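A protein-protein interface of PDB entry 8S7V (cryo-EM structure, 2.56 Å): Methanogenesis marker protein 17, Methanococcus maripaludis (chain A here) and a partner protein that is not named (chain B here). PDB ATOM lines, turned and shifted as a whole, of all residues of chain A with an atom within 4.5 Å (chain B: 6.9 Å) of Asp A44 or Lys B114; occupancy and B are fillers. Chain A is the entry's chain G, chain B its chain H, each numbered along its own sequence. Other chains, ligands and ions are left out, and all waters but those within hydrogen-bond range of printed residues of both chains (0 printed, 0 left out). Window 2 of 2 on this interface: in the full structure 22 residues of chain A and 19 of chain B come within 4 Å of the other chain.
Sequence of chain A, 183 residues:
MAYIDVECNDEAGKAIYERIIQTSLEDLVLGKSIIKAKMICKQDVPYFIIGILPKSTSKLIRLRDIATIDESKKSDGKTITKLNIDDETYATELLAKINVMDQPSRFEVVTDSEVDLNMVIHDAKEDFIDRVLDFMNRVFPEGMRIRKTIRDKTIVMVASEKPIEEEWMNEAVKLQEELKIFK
Among the printed residues, merely in contact across the chains: Gln A43 with Ser B142 and Pro A46 with Lys B114.
Of the 13 printed residues of chain B, 3 touch a printed residue of chain A.
Printed residues of chain B that touch a printed residue of chain A: Lys B114, Asn B115 and Ser B142.
Of the 6 printed residues of chain A, 4 touch a printed residue of chain B.
Hydrophobic or aromatic side chains of chain A within 4 Å of the printed part of chain B: Pro A46.
Along chain A the printed residues that touch a printed residue of chain B span positions 43 to 161.
Among the printed residues, no Asp or Glu carboxylate lies within 4 Å of a Lys or Arg side-chain nitrogen of the other chain.
Lys A42 touches none of the printed residues of chain B.
Printed residues of chain B within 4 Å of Gln A43: Lys B114 (2.4 Å) and Ser B142 (3.6 Å).
Of chain B, only Lys B114 comes within 4 Å of Asp A44.
Printed residues of chain B within 4 Å of Pro A46: Lys B114 (3.6 Å).
Gly B113 touches none of the printed residues of chain A.
Lys B114 touches just these residues of chain A: Gln A43 (2.4 Å), Asp A44 (3.3 Å), Pro A46 (3.6 Å) and Glu A161 (3.3 Å).
The nearest printed residue of chain A that does not touch Lys B114 is Val A45 (4.7 Å).
The side-chain amino group of Lys B114 lies within hydrogen-bond range of the side-chain hydroxyl of Ser B142, 2.7 Å away.
OD1 of Asn B115 sits close to OD2 of Asp B146 (2.9 Å).
The backbone carbonyl oxygen (O) of Gln A43 sits at hydrogen-bond distance from the side-chain amino group (NZ) of Lys B114 (2.4 Å).
NZ of Lys B114 lies within hydrogen-bond range of O of Asp A44, at 3.3 Å.
OE1 of Glu A161 is in hydrogen-bond range of N of Lys B114 (3.3 Å).
The side-chain carboxylate (OE2) of Glu A161 lies within hydrogen-bond range of the side-chain amide nitrogen (ND2) of Asn B115 (3.1 Å).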
ATOM      1  N   LYS A  42      26.208   5.379  -0.245  1.00  0.00           N
ATOM      2  CA  LYS A  42      26.858   6.565   0.301  1.00  0.00           C
ATOM      3  C   LYS A  42      27.101   7.521  -0.858  1.00  0.00           C
ATOM      4  O   LYS A  42      28.044   7.337  -1.634  1.00  0.00           O
ATOM      5  CB  LYS A  42      28.162   6.204   1.009  1.00  0.00           C
ATOM      6  CG  LYS A  42      27.997   5.189   2.124  1.00  0.00           C
ATOM      7  CD  LYS A  42      28.180   5.831   3.488  1.00  0.00           C
ATOM      8  CE  LYS A  42      27.288   5.174   4.528  1.00  0.00           C
ATOM      9  NZ  LYS A  42      25.930   5.784   4.559  1.00  0.00           N
ATOM     10  N   GLN A  43      26.238   8.529  -0.990  1.00  0.00           N
ATOM     11  CA  GLN A  43      26.326   9.471  -2.095  1.00  0.00           C
ATOM     12  C   GLN A  43      27.050  10.763  -1.751  1.00  0.00           C
ATOM     13  O   GLN A  43      27.581  11.407  -2.660  1.00  0.00           O
ATOM     14  CB  GLN A  43      24.924   9.810  -2.621  1.00  0.00           C
ATOM     15  CG  GLN A  43      24.009  10.436  -1.590  1.00  0.00           C
ATOM     16  CD  GLN A  43      23.063   9.428  -0.976  1.00  0.00           C
ATOM     17  OE1 GLN A  43      23.281   8.221  -1.069  1.00  0.00           O
ATOM     18  NE2 GLN A  43      22.005   9.917  -0.343  1.00  0.00           N
ATOM     19  N   ASP A  44      27.080  11.161  -0.477  1.00  0.00           N
ATOM     20  CA  ASP A  44      27.819  12.362  -0.100  1.00  0.00           C
ATOM     21  C   ASP A  44      29.305  12.196  -0.389  1.00  0.00           C
ATOM     22  O   ASP A  44      29.941  13.086  -0.963  1.00  0.00           O
ATOM     23  CB  ASP A  44      27.577  12.682   1.373  1.00  0.00           C
ATOM     24  CG  ASP A  44      26.103  12.810   1.702  1.00  0.00           C
ATOM     25  OD1 ASP A  44      25.287  12.127   1.049  1.00  0.00           O
ATOM     26  OD2 ASP A  44      25.759  13.594   2.611  1.00  0.00           O
ATOM     27  N   VAL A  45      29.872  11.062   0.001  1.00  0.00           N
ATOM     28  CA  VAL A  45      31.174  10.608  -0.475  1.00  0.00           C
ATOM     29  C   VAL A  45      30.911   9.479  -1.465  1.00  0.00           C
ATOM     30  O   VAL A  45      30.445   8.407  -1.060  1.00  0.00           O
ATOM     31  CB  VAL A  45      32.079  10.144   0.679  1.00  0.00           C
ATOM     32  CG1 VAL A  45      31.263   9.451   1.765  1.00  0.00           C
ATOM     33  CG2 VAL A  45      33.192   9.238   0.162  1.00  0.00           C
ATOM     34  N   PRO A  46      31.175   9.668  -2.754  1.00  0.00           N
ATOM     35  CA  PRO A  46      30.638   8.736  -3.753  1.00  0.00           C
ATOM     36  C   PRO A  46      31.264   7.355  -3.675  1.00  0.00           C
ATOM     37  O   PRO A  46      32.401   7.148  -4.109  1.00  0.00           O
ATOM     38  CB  PRO A  46      30.966   9.420  -5.089  1.00  0.00           C
ATOM     39  CG  PRO A  46      31.320  10.832  -4.739  1.00  0.00           C
ATOM     40  CD  PRO A  46      31.904  10.784  -3.373  1.00  0.00           C
ATOM     41  N   GLU A 161      34.095   6.575  -7.854  1.00  0.00           N
ATOM     42  CA  GLU A 161      34.791   7.331  -8.885  1.00  0.00           C
ATOM     43  C   GLU A 161      36.219   7.672  -8.486  1.00  0.00           C
ATOM     44  O   GLU A 161      37.005   8.094  -9.341  1.00  0.00           O
ATOM     45  CB  GLU A 161      34.030   8.618  -9.205  1.00  0.00           C
ATOM     46  CG  GLU A 161      34.262   9.738  -8.206  1.00  0.00           C
ATOM     47  CD  GLU A 161      33.036  10.603  -8.002  1.00  0.00           C
ATOM     48  OE1 GLU A 161      31.974  10.276  -8.572  1.00  0.00           O
ATOM     49  OE2 GLU A 161      33.137  11.614  -7.276  1.00  0.00           O
ATOM     50  N   GLY B 111      29.116  13.080 -18.931  1.00  0.00           N
ATOM     51  CA  GLY B 111      27.976  13.462 -18.127  1.00  0.00           C
ATOM     52  C   GLY B 111      27.739  12.642 -16.882  1.00  0.00           C
ATOM     53  O   GLY B 111      26.862  12.985 -16.087  1.00  0.00           O
ATOM     54  N   ALA B 112      28.496  11.569 -16.678  1.00  0.00           N
ATOM     55  CA  ALA B 112      28.287  10.669 -15.555  1.00  0.00           C
ATOM     56  C   ALA B 112      29.244  10.995 -14.418  1.00  0.00           C
ATOM     57  O   ALA B 112      30.287  11.623 -14.616  1.00  0.00           O
ATOM     58  CB  ALA B 112      28.466   9.214 -15.985  1.00  0.00           C
ATOM     59  N   GLY B 113      28.879  10.555 -13.219  1.00  0.00           N
ATOM     60  CA  GLY B 113      29.652  10.822 -12.025  1.00  0.00           C
ATOM     61  C   GLY B 113      29.071  11.967 -11.212  1.00  0.00           C
ATOM     62  O   GLY B 113      28.079  12.600 -11.578  1.00  0.00           O
ATOM     63  N   LYS B 114      29.713  12.225 -10.075  1.00  0.00           N
ATOM     64  CA  LYS B 114      29.302  13.303  -9.184  1.00  0.00           C
ATOM     65  C   LYS B 114      30.151  14.555  -9.353  1.00  0.00           C
ATOM     66  O   LYS B 114      29.619  15.633  -9.628  1.00  0.00           O
ATOM     67  CB  LYS B 114      29.353  12.829  -7.727  1.00  0.00           C
ATOM     68  CG  LYS B 114      28.572  13.710  -6.771  1.00  0.00           C
ATOM     69  CD  LYS B 114      28.667  13.202  -5.345  1.00  0.00           C
ATOM     70  CE  LYS B 114      28.364  14.305  -4.348  1.00  0.00           C
ATOM     71  NZ  LYS B 114      27.644  13.786  -3.155  1.00  0.00           N
ATOM     72  N   ASN B 115      31.469  14.436  -9.193  1.00  0.00           N
ATOM     73  CA  ASN B 115      32.374  15.562  -9.354  1.00  0.00           C
ATOM     74  C   ASN B 115      33.203  15.493 -10.626  1.00  0.00           C
ATOM     75  O   ASN B 115      33.960  16.429 -10.902  1.00  0.00           O
ATOM     76  CB  ASN B 115      33.318  15.662  -8.146  1.00  0.00           C
ATOM     77  CG  ASN B 115      32.632  15.314  -6.842  1.00  0.00           C
ATOM     78  OD1 ASN B 115      31.555  15.826  -6.538  1.00  0.00           O
ATOM     79  ND2 ASN B 115      33.254  14.438  -6.062  1.00  0.00           N
ATOM     80  N   ILE B 116      33.087  14.419 -11.402  1.00  0.00           N
ATOM     81  CA  ILE B 116      33.881  14.250 -12.614  1.00  0.00           C
ATOM     82  C   ILE B 116      33.015  14.521 -13.836  1.00  0.00           C
ATOM     83  O   ILE B 116      33.446  14.308 -14.975  1.00  0.00           O
ATOM     84  CB  ILE B 116      34.503  12.844 -12.676  1.00  0.00           C
ATOM     85  CG1 ILE B 116      33.430  11.775 -12.462  1.00  0.00           C
ATOM     86  CG2 ILE B 116      35.606  12.707 -11.642  1.00  0.00           C
ATOM     87  CD1 ILE B 116      33.828  10.405 -12.962  1.00  0.00           C
ATOM     88  N   SER B 117      31.792  14.994 -13.611  1.00  0.00           N
ATOM     89  CA  SER B 117      30.891  15.300 -14.712  1.00  0.00           C
ATOM     90  C   SER B 117      31.225  16.658 -15.312  1.00  0.00           C
ATOM     91  O   SER B 117      31.500  17.624 -14.593  1.00  0.00           O
ATOM     92  CB  SER B 117      29.439  15.283 -14.239  1.00  0.00           C
ATOM     93  OG  SER B 117      29.223  16.246 -13.224  1.00  0.00           O
ATOM     94  N   SER B 142      21.906  14.892  -3.337  1.00  0.00           N
ATOM     95  CA  SER B 142      23.238  15.486  -3.282  1.00  0.00           C
ATOM     96  C   SER B 142      23.934  15.437  -4.636  1.00  0.00           C
ATOM     97  O   SER B 142      24.585  16.411  -5.033  1.00  0.00           O
ATOM     98  CB  SER B 142      24.087  14.781  -2.227  1.00  0.00           C
ATOM     99  OG  SER B 142      24.938  13.818  -2.821  1.00  0.00           O
ATOM    100  N   CYS B 143      23.809  14.319  -5.354  1.00  0.00           N
ATOM    101  CA  CYS B 143      24.451  14.195  -6.657  1.00  0.00           C
ATOM    102  C   CYS B 143      23.902  15.223  -7.638  1.00  0.00           C
ATOM    103  O   CYS B 143      24.661  15.859  -8.377  1.00  0.00           O
ATOM    104  CB  CYS B 143      24.267  12.777  -7.197  1.00  0.00           C
ATOM    105  SG  CYS B 143      25.370  11.550  -6.463  1.00  0.00           S
ATOM    106  N   ILE B 144      22.579  15.400  -7.658  1.00  0.00           N
ATOM    107  CA  ILE B 144      21.981  16.395  -8.542  1.00  0.00           C
ATOM    108  C   ILE B 144      22.373  17.805  -8.122  1.00  0.00           C
ATOM    109  O   ILE B 144      22.699  18.645  -8.970  1.00  0.00           O
ATOM    110  CB  ILE B 144      20.451  16.229  -8.591  1.00  0.00           C
ATOM    111  CG1 ILE B 144      20.082  14.827  -9.072  1.00  0.00           C
ATOM    112  CG2 ILE B 144      19.823  17.284  -9.485  1.00  0.00           C
ATOM    113  CD1 ILE B 144      18.609  14.518  -8.968  1.00  0.00           C
ATOM    114  N   ASP B 146      25.037  18.773  -6.695  1.00  0.00           N
ATOM    115  CA  ASP B 146      26.433  18.979  -7.049  1.00  0.00           C
ATOM    116  C   ASP B 146      26.655  18.746  -8.547  1.00  0.00           C
ATOM    117  O   ASP B 146      27.730  18.306  -8.964  1.00  0.00           O
ATOM    118  CB  ASP B 146      27.313  18.059  -6.186  1.00  0.00           C
ATOM    119  CG  ASP B 146      28.814  18.306  -6.350  1.00  0.00           C
ATOM    120  OD1 ASP B 146      29.233  19.155  -7.162  1.00  0.00           O
ATOM    121  OD2 ASP B 146      29.584  17.699  -5.576  1.00  0.00           O
ATOM    122  N   LYS B 147      25.627  18.991  -9.363  1.00  0.00           N
ATOM    123  CA  LYS B 147      25.700  18.770 -10.802  1.00  0.00           C
ATOM    124  C   LYS B 147      25.024  19.903 -11.565  1.00  0.00           C
ATOM    125  O   LYS B 147      24.669  19.741 -12.737  1.00  0.00           O
ATOM    126  CB  LYS B 147      25.063  17.430 -11.174  1.00  0.00           C
ATOM    127  CG  LYS B 147      25.832  16.627 -12.206  1.00  0.00           C
ATOM    128  CD  LYS B 147      25.135  15.306 -12.485  1.00  0.00           C
ATOM    129  CE  LYS B 147      26.041  14.346 -13.231  1.00  0.00           C
ATOM    130  NZ  LYS B 147      25.576  12.939 -13.107  1.00  0.00           N
ATOM    131  N   HIS B 149      26.140  22.637 -12.772  1.00  0.00           N
ATOM    132  CA  HIS B 149      26.893  23.198 -13.889  1.00  0.00           C
ATOM    133  C   HIS B 149      26.550  22.537 -15.216  1.00  0.00           C
ATOM    134  O   HIS B 149      26.854  23.101 -16.273  1.00  0.00           O
ATOM    135  CB  HIS B 149      28.393  23.086 -13.613  1.00  0.00           C
ATOM    136  CG  HIS B 149      28.916  21.685 -13.671  1.00  0.00           C
ATOM    137  ND1 HIS B 149      28.454  20.684 -12.845  1.00  0.00           N
ATOM    138  CD2 HIS B 149      29.868  21.120 -14.451  1.00  0.00           C
ATOM    139  CE1 HIS B 149      29.095  19.561 -13.116  1.00  0.00           C
ATOM    140  NE2 HIS B 149      29.960  19.800 -14.086  1.00  0.00           N
